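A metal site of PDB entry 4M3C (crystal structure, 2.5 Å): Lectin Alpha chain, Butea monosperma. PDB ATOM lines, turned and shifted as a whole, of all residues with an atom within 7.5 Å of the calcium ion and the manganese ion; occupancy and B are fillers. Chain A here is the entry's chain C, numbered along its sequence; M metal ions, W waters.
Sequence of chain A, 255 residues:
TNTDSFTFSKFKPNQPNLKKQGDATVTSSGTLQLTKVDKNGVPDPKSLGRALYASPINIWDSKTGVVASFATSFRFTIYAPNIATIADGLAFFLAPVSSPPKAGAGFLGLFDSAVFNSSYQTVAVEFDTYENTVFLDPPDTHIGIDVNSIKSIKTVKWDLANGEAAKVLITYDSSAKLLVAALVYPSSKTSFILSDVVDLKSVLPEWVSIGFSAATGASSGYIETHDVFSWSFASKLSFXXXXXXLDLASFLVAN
Ser 152 touches the manganese ion (OG to MN, 3.9 Å).
Within 4 Å of the calcium ion: Asp 128, Tyr 130, Asn 132 and Asp 137.
The nearest printed residue that does not touch the calcium ion is Gly 106 (4.5 Å).
Water W1 lies within hydrogen-bond range of O of Ile 150 (2.5 Å) and OE1 of Glu 126 (2.9 Å).
Water W3 is bound to the calcium ion.
The side-chain carboxylate (OD2) of Asp 137 binds the calcium ion, 2.1 Å away.
The backbone carbonyl oxygen (O) of Tyr 130 is bound to the calcium ion.
The calcium ion is bound by OD1 of Asp 128, 2.5 Å away.
The calcium ion is bound by OD1 of Asn 132 (2.6 Å).
Water W2 binds the calcium ion, 2.6 Å away.
The calcium ion is bound by OD2 of Asp 128 (2.7 Å).
The calcium ion has seven donor atoms within binding distance.
OE1 of Glu 126 sits close to OD2 of Asp 146 (2.6 Å).
The side-chain hydroxyl (OG) of Ser 152 is in hydrogen-bond range of the side-chain carboxylate (OD1) of Asp 146 (2.7 Å).
The backbone NH (N) of Glu 126 lies within hydrogen-bond range of the backbone carbonyl oxygen (O) of Gly 144 (2.9 Å).
The side-chain hydroxyl (OG) of Ser 152 sits close to the side-chain carboxylate (OE2) of Glu 126 (3.5 Å).
ND1 of His 142 lies within hydrogen-bond range of O of Asp 140 (2.7 Å).
The manganese ion is bound by water W4 (1.9 Å), the side-chain carboxylate (OD2) of Asp 128 (2.0 Å), the side-chain carboxylate (OE2) of Glu 126 (2.2 Å), the side-chain carboxylate (OD1) of Asp 137 (2.2 Å), a ring nitrogen (NE2) of His 142 (2.4 Å) and water W1 (2.6 Å).
The manganese ion has six donor atoms within binding distance.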
ATOM      1  N   ASP A  88     -21.773  17.486   6.733  1.00  0.00           N
ATOM      2  CA  ASP A  88     -22.285  16.279   7.367  1.00  0.00           C
ATOM      3  C   ASP A  88     -22.273  15.039   6.480  1.00  0.00           C
ATOM      4  O   ASP A  88     -22.281  13.912   6.996  1.00  0.00           O
ATOM      5  CB  ASP A  88     -23.713  16.492   7.805  1.00  0.00           C
ATOM      6  CG  ASP A  88     -23.814  16.996   9.223  1.00  0.00           C
ATOM      7  OD1 ASP A  88     -24.098  18.201   9.429  1.00  0.00           O
ATOM      8  OD2 ASP A  88     -23.631  16.176  10.126  1.00  0.00           O
ATOM      9  N   GLY A  89     -22.299  15.228   5.173  1.00  0.00           N
ATOM     10  CA  GLY A  89     -22.295  14.085   4.272  1.00  0.00           C
ATOM     11  C   GLY A  89     -22.982  14.333   2.948  1.00  0.00           C
ATOM     12  O   GLY A  89     -23.553  15.387   2.730  1.00  0.00           O
ATOM     13  N   ALA A 105     -28.362  19.085   7.954  1.00  0.00           N
ATOM     14  CA  ALA A 105     -27.389  18.447   8.843  1.00  0.00           C
ATOM     15  C   ALA A 105     -27.321  16.915   8.730  1.00  0.00           C
ATOM     16  O   ALA A 105     -27.491  16.340   7.647  1.00  0.00           O
ATOM     17  CB  ALA A 105     -27.633  18.875  10.291  1.00  0.00           C
ATOM     18  N   GLY A 106     -27.076  16.247   9.860  1.00  0.00           N
ATOM     19  CA  GLY A 106     -26.948  14.788   9.876  1.00  0.00           C
ATOM     20  C   GLY A 106     -28.078  13.944   9.296  1.00  0.00           C
ATOM     21  O   GLY A 106     -27.956  12.719   9.265  1.00  0.00           O
ATOM     22  N   PHE A 107     -29.151  14.593   8.865  1.00  0.00           N
ATOM     23  CA  PHE A 107     -30.315  13.924   8.229  1.00  0.00           C
ATOM     24  C   PHE A 107     -30.088  13.964   6.710  1.00  0.00           C
ATOM     25  O   PHE A 107     -30.740  13.250   5.976  1.00  0.00           O
ATOM     26  CB  PHE A 107     -31.646  14.660   8.531  1.00  0.00           C
ATOM     27  CG  PHE A 107     -31.904  14.953   9.984  1.00  0.00           C
ATOM     28  CD1 PHE A 107     -32.530  14.021  10.800  1.00  0.00           C
ATOM     29  CD2 PHE A 107     -31.581  16.194  10.533  1.00  0.00           C
ATOM     30  CE1 PHE A 107     -32.773  14.283  12.135  1.00  0.00           C
ATOM     31  CE2 PHE A 107     -31.833  16.465  11.863  1.00  0.00           C
ATOM     32  CZ  PHE A 107     -32.425  15.509  12.673  1.00  0.00           C
ATOM     33  N   LEU A 108     -29.193  14.860   6.274  1.00  0.00           N
ATOM     34  CA  LEU A 108     -28.686  14.884   4.898  1.00  0.00           C
ATOM     35  C   LEU A 108     -29.779  15.200   3.873  1.00  0.00           C
ATOM     36  O   LEU A 108     -29.719  14.775   2.719  1.00  0.00           O
ATOM     37  CB  LEU A 108     -27.954  13.570   4.532  1.00  0.00           C
ATOM     38  CG  LEU A 108     -26.933  12.960   5.505  1.00  0.00           C
ATOM     39  CD1 LEU A 108     -26.346  11.659   4.968  1.00  0.00           C
ATOM     40  CD2 LEU A 108     -25.813  13.935   5.839  1.00  0.00           C
ATOM     41  N   GLU A 126     -25.349   6.406   1.812  1.00  0.00           N
ATOM     42  CA  GLU A 126     -24.870   7.624   2.419  1.00  0.00           C
ATOM     43  C   GLU A 126     -23.341   7.604   2.609  1.00  0.00           C
ATOM     44  O   GLU A 126     -22.750   6.560   2.897  1.00  0.00           O
ATOM     45  CB  GLU A 126     -25.594   7.856   3.743  1.00  0.00           C
ATOM     46  CG  GLU A 126     -25.124   6.953   4.862  1.00  0.00           C
ATOM     47  CD  GLU A 126     -25.477   7.495   6.227  1.00  0.00           C
ATOM     48  OE1 GLU A 126     -26.561   8.074   6.381  1.00  0.00           O
ATOM     49  OE2 GLU A 126     -24.667   7.327   7.142  1.00  0.00           O
ATOM     50  N   PHE A 127     -22.737   8.762   2.429  1.00  0.00           N
ATOM     51  CA  PHE A 127     -21.309   8.944   2.623  1.00  0.00           C
ATOM     52  C   PHE A 127     -21.269   9.991   3.698  1.00  0.00           C
ATOM     53  O   PHE A 127     -21.501  11.175   3.440  1.00  0.00           O
ATOM     54  CB  PHE A 127     -20.637   9.393   1.328  1.00  0.00           C
ATOM     55  CG  PHE A 127     -20.923   8.483   0.203  1.00  0.00           C
ATOM     56  CD1 PHE A 127     -20.167   7.348  -0.003  1.00  0.00           C
ATOM     57  CD2 PHE A 127     -22.054   8.673  -0.580  1.00  0.00           C
ATOM     58  CE1 PHE A 127     -20.478   6.467  -0.996  1.00  0.00           C
ATOM     59  CE2 PHE A 127     -22.373   7.781  -1.593  1.00  0.00           C
ATOM     60  CZ  PHE A 127     -21.581   6.669  -1.787  1.00  0.00           C
ATOM     61  N   ASP A 128     -20.964   9.515   4.900  1.00  0.00           N
ATOM     62  CA  ASP A 128     -21.259  10.242   6.112  1.00  0.00           C
ATOM     63  C   ASP A 128     -19.974  10.671   6.860  1.00  0.00           C
ATOM     64  O   ASP A 128     -19.246   9.846   7.423  1.00  0.00           O
ATOM     65  CB  ASP A 128     -22.183   9.342   6.956  1.00  0.00           C
ATOM     66  CG  ASP A 128     -22.668  10.002   8.216  1.00  0.00           C
ATOM     67  OD1 ASP A 128     -22.359  11.201   8.473  1.00  0.00           O
ATOM     68  OD2 ASP A 128     -23.384   9.306   8.984  1.00  0.00           O
ATOM     69  N   THR A 129     -19.752  11.989   6.909  1.00  0.00           N
ATOM     70  CA  THR A 129     -18.522  12.510   7.477  1.00  0.00           C
ATOM     71  C   THR A 129     -18.531  12.985   8.943  1.00  0.00           C
ATOM     72  O   THR A 129     -17.483  13.407   9.464  1.00  0.00           O
ATOM     73  CB  THR A 129     -17.898  13.575   6.575  1.00  0.00           C
ATOM     74  OG1 THR A 129     -18.797  14.699   6.402  1.00  0.00           O
ATOM     75  CG2 THR A 129     -17.573  12.948   5.228  1.00  0.00           C
ATOM     76  N   TYR A 130     -19.656  12.868   9.627  1.00  0.00           N
ATOM     77  CA  TYR A 130     -19.744  13.420  10.994  1.00  0.00           C
ATOM     78  C   TYR A 130     -20.554  12.539  11.939  1.00  0.00           C
ATOM     79  O   TYR A 130     -21.670  12.179  11.614  1.00  0.00           O
ATOM     80  CB  TYR A 130     -20.313  14.851  10.974  1.00  0.00           C
ATOM     81  CG  TYR A 130     -20.621  15.364  12.362  1.00  0.00           C
ATOM     82  CD1 TYR A 130     -19.641  15.999  13.136  1.00  0.00           C
ATOM     83  CD2 TYR A 130     -21.873  15.165  12.941  1.00  0.00           C
ATOM     84  CE1 TYR A 130     -19.903  16.420  14.417  1.00  0.00           C
ATOM     85  CE2 TYR A 130     -22.152  15.588  14.217  1.00  0.00           C
ATOM     86  CZ  TYR A 130     -21.167  16.211  14.966  1.00  0.00           C
ATOM     87  OH  TYR A 130     -21.451  16.622  16.232  1.00  0.00           O
ATOM     88  N   GLU A 131     -19.995  12.210  13.093  1.00  0.00           N
ATOM     89  CA  GLU A 131     -20.666  11.291  14.013  1.00  0.00           C
ATOM     90  C   GLU A 131     -21.866  11.923  14.778  1.00  0.00           C
ATOM     91  O   GLU A 131     -21.687  12.781  15.643  1.00  0.00           O
ATOM     92  CB  GLU A 131     -19.694  10.648  15.000  1.00  0.00           C
ATOM     93  CG  GLU A 131     -20.313   9.470  15.710  1.00  0.00           C
ATOM     94  CD  GLU A 131     -19.480   8.895  16.843  1.00  0.00           C
ATOM     95  OE1 GLU A 131     -18.574   9.581  17.372  1.00  0.00           O
ATOM     96  OE2 GLU A 131     -19.755   7.739  17.215  1.00  0.00           O
ATOM     97  N   ASN A 132     -23.080  11.486  14.444  1.00  0.00           N
ATOM     98  CA  ASN A 132     -24.252  11.806  15.225  1.00  0.00           C
ATOM     99  C   ASN A 132     -24.583  10.551  15.989  1.00  0.00           C
ATOM    100  O   ASN A 132     -25.119   9.599  15.413  1.00  0.00           O
ATOM    101  CB  ASN A 132     -25.438  12.247  14.361  1.00  0.00           C
ATOM    102  CG  ASN A 132     -25.093  13.380  13.411  1.00  0.00           C
ATOM    103  OD1 ASN A 132     -24.465  13.159  12.371  1.00  0.00           O
ATOM    104  ND2 ASN A 132     -25.528  14.618  13.753  1.00  0.00           N
ATOM    105  N   THR A 133     -24.227  10.553  17.280  1.00  0.00           N
ATOM    106  CA  THR A 133     -24.445   9.425  18.207  1.00  0.00           C
ATOM    107  C   THR A 133     -25.943   9.160  18.402  1.00  0.00           C
ATOM    108  O   THR A 133     -26.367   8.004  18.538  1.00  0.00           O
ATOM    109  CB  THR A 133     -23.806   9.682  19.595  1.00  0.00           C
ATOM    110  OG1 THR A 133     -22.387   9.776  19.456  1.00  0.00           O
ATOM    111  CG2 THR A 133     -24.148   8.567  20.633  1.00  0.00           C
ATOM    112  N   PHE A 135     -27.941   9.063  16.126  1.00  0.00           N
ATOM    113  CA  PHE A 135     -28.329   8.215  14.984  1.00  0.00           C
ATOM    114  C   PHE A 135     -27.632   6.851  14.935  1.00  0.00           C
ATOM    115  O   PHE A 135     -27.853   6.064  13.989  1.00  0.00           O
ATOM    116  CB  PHE A 135     -28.116   8.929  13.640  1.00  0.00           C
ATOM    117  CG  PHE A 135     -28.759  10.300  13.530  1.00  0.00           C
ATOM    118  CD1 PHE A 135     -29.939  10.632  14.208  1.00  0.00           C
ATOM    119  CD2 PHE A 135     -28.209  11.245  12.669  1.00  0.00           C
ATOM    120  CE1 PHE A 135     -30.527  11.892  14.082  1.00  0.00           C
ATOM    121  CE2 PHE A 135     -28.783  12.504  12.537  1.00  0.00           C
ATOM    122  CZ  PHE A 135     -29.940  12.832  13.239  1.00  0.00           C
ATOM    123  N   LEU A 136     -26.808   6.557  15.944  1.00  0.00           N
ATOM    124  CA  LEU A 136     -25.984   5.338  16.011  1.00  0.00           C
ATOM    125  C   LEU A 136     -24.874   5.342  14.916  1.00  0.00           C
ATOM    126  O   LEU A 136     -24.345   4.292  14.537  1.00  0.00           O
ATOM    127  CB  LEU A 136     -26.839   4.033  16.067  1.00  0.00           C
ATOM    128  CG  LEU A 136     -26.358   2.589  16.440  1.00  0.00           C
ATOM    129  CD1 LEU A 136     -26.182   1.661  15.219  1.00  0.00           C
ATOM    130  CD2 LEU A 136     -25.178   2.456  17.429  1.00  0.00           C
ATOM    131  N   ASP A 137     -24.509   6.543  14.454  1.00  0.00           N
ATOM    132  CA  ASP A 137     -23.245   6.723  13.728  1.00  0.00           C
ATOM    133  C   ASP A 137     -22.063   6.124  14.483  1.00  0.00           C
ATOM    134  O   ASP A 137     -21.936   6.334  15.663  1.00  0.00           O
ATOM    135  CB  ASP A 137     -22.958   8.185  13.485  1.00  0.00           C
ATOM    136  CG  ASP A 137     -23.619   8.693  12.235  1.00  0.00           C
ATOM    137  OD1 ASP A 137     -24.205   7.864  11.513  1.00  0.00           O
ATOM    138  OD2 ASP A 137     -23.551   9.945  11.943  1.00  0.00           O
ATOM    139  N   PRO A 138     -21.213   5.348  13.770  1.00  0.00           N
ATOM    140  CA  PRO A 138     -19.894   4.915  14.285  1.00  0.00           C
ATOM    141  C   PRO A 138     -18.902   6.070  14.414  1.00  0.00           C
ATOM    142  O   PRO A 138     -19.128   7.137  13.824  1.00  0.00           O
ATOM    143  CB  PRO A 138     -19.400   3.926  13.196  1.00  0.00           C
ATOM    144  CG  PRO A 138     -20.256   4.167  12.008  1.00  0.00           C
ATOM    145  CD  PRO A 138     -21.575   4.669  12.515  1.00  0.00           C
ATOM    146  N   ASP A 140     -16.250   6.699  13.013  1.00  0.00           N
ATOM    147  CA  ASP A 140     -15.367   6.904  11.850  1.00  0.00           C
ATOM    148  C   ASP A 140     -16.225   7.364  10.686  1.00  0.00           C
ATOM    149  O   ASP A 140     -17.427   7.048  10.646  1.00  0.00           O
ATOM    150  CB  ASP A 140     -14.524   5.645  11.527  1.00  0.00           C
ATOM    151  CG  ASP A 140     -15.330   4.330  11.574  1.00  0.00           C
ATOM    152  OD1 ASP A 140     -16.079   4.025  10.606  1.00  0.00           O
ATOM    153  OD2 ASP A 140     -15.170   3.537  12.554  1.00  0.00           O
ATOM    154  N   HIS A 142     -17.879   7.077   7.275  1.00  0.00           N
ATOM    155  CA  HIS A 142     -18.398   5.778   6.896  1.00  0.00           C
ATOM    156  C   HIS A 142     -19.298   5.829   5.716  1.00  0.00           C
ATOM    157  O   HIS A 142     -19.718   6.907   5.296  1.00  0.00           O
ATOM    158  CB  HIS A 142     -19.092   5.115   8.080  1.00  0.00           C
ATOM    159  CG  HIS A 142     -20.183   5.953   8.708  1.00  0.00           C
ATOM    160  ND1 HIS A 142     -19.959   6.778   9.756  1.00  0.00           N
ATOM    161  CD2 HIS A 142     -21.539   6.086   8.397  1.00  0.00           C
ATOM    162  CE1 HIS A 142     -21.099   7.405  10.099  1.00  0.00           C
ATOM    163  NE2 HIS A 142     -22.067   6.984   9.268  1.00  0.00           N
ATOM    164  N   ILE A 143     -19.570   4.664   5.150  1.00  0.00           N
ATOM    165  CA  ILE A 143     -20.568   4.508   4.102  1.00  0.00           C
ATOM    166  C   ILE A 143     -21.628   3.690   4.793  1.00  0.00           C
ATOM    167  O   ILE A 143     -21.307   2.859   5.665  1.00  0.00           O
ATOM    168  CB  ILE A 143     -19.992   3.732   2.898  1.00  0.00           C
ATOM    169  CG1 ILE A 143     -18.986   4.617   2.173  1.00  0.00           C
ATOM    170  CG2 ILE A 143     -21.076   3.282   1.923  1.00  0.00           C
ATOM    171  CD1 ILE A 143     -18.015   3.809   1.325  1.00  0.00           C
ATOM    172  N   GLY A 144     -22.880   3.944   4.463  1.00  0.00           N
ATOM    173  CA  GLY A 144     -23.979   3.233   5.120  1.00  0.00           C
ATOM    174  C   GLY A 144     -25.201   3.108   4.235  1.00  0.00           C
ATOM    175  O   GLY A 144     -25.412   3.945   3.335  1.00  0.00           O
ATOM    176  N   ASP A 146     -29.192   3.248   4.137  1.00  0.00           N
ATOM    177  CA  ASP A 146     -30.304   3.906   4.852  1.00  0.00           C
ATOM    178  C   ASP A 146     -31.629   3.478   4.237  1.00  0.00           C
ATOM    179  O   ASP A 146     -31.875   3.725   3.042  1.00  0.00           O
ATOM    180  CB  ASP A 146     -30.177   5.429   4.699  1.00  0.00           C
ATOM    181  CG  ASP A 146     -29.046   6.010   5.559  1.00  0.00           C
ATOM    182  OD1 ASP A 146     -28.417   5.230   6.359  1.00  0.00           O
ATOM    183  OD2 ASP A 146     -28.798   7.245   5.446  1.00  0.00           O
ATOM    184  N   ILE A 150     -32.365   7.177   9.153  1.00  0.00           N
ATOM    185  CA  ILE A 150     -31.012   7.643   9.129  1.00  0.00           C
ATOM    186  C   ILE A 150     -30.118   6.742  10.006  1.00  0.00           C
ATOM    187  O   ILE A 150     -28.909   6.852   9.968  1.00  0.00           O
ATOM    188  CB  ILE A 150     -30.909   9.107   9.546  1.00  0.00           C
ATOM    189  CG1 ILE A 150     -29.534   9.676   9.185  1.00  0.00           C
ATOM    190  CG2 ILE A 150     -31.185   9.233  11.034  1.00  0.00           C
ATOM    191  CD1 ILE A 150     -29.391  10.115   7.748  1.00  0.00           C
ATOM    192  N   LYS A 151     -30.718   5.852  10.808  1.00  0.00           N
ATOM    193  CA  LYS A 151     -29.953   4.832  11.477  1.00  0.00           C
ATOM    194  C   LYS A 151     -29.614   3.703  10.477  1.00  0.00           C
ATOM    195  O   LYS A 151     -30.380   2.749  10.339  1.00  0.00           O
ATOM    196  CB  LYS A 151     -30.710   4.273  12.679  1.00  0.00           C
ATOM    197  CG  LYS A 151     -30.744   5.181  13.899  1.00  0.00           C
ATOM    198  CD  LYS A 151     -30.990   4.383  15.188  1.00  0.00           C
ATOM    199  CE  LYS A 151     -31.658   5.232  16.276  1.00  0.00           C
ATOM    200  NZ  LYS A 151     -33.158   5.134  16.218  1.00  0.00           N
ATOM    201  N   SER A 152     -28.475   3.820   9.787  1.00  0.00           N
ATOM    202  CA  SER A 152     -28.122   2.899   8.717  1.00  0.00           C
ATOM    203  C   SER A 152     -28.300   1.425   9.091  1.00  0.00           C
ATOM    204  O   SER A 152     -27.734   0.958  10.080  1.00  0.00           O
ATOM    205  CB  SER A 152     -26.660   3.117   8.291  1.00  0.00           C
ATOM    206  OG  SER A 152     -26.423   4.482   8.052  1.00  0.00           O
ATOM    207  N   THR A 155     -23.151  -0.539   7.909  1.00  0.00           N
ATOM    208  CA  THR A 155     -22.069   0.429   7.556  1.00  0.00           C
ATOM    209  C   THR A 155     -20.659  -0.186   7.310  1.00  0.00           C
ATOM    210  O   THR A 155     -20.401  -1.381   7.577  1.00  0.00           O
ATOM    211  CB  THR A 155     -21.912   1.553   8.611  1.00  0.00           C
ATOM    212  OG1 THR A 155     -21.251   1.059   9.798  1.00  0.00           O
ATOM    213  CG2 THR A 155     -23.250   2.195   8.986  1.00  0.00           C
HETATM  214 CA    CA M   1     -23.825  11.508  10.533  1.00  0.00          CA
HETATM  215 MN    MN M   2     -24.423   7.622   9.306  1.00  0.00          MN
HETATM  216  O   HOH W   1     -26.945   8.140   9.223  1.00  0.00           O
HETATM  217  O   HOH W   2     -25.809  10.277   9.399  1.00  0.00           O
HETATM  218  O   HOH W   3     -23.793  13.330   9.762  1.00  0.00           O
HETATM  219  O   HOH W   4     -24.890   5.780   9.706  1.00  0.00           O
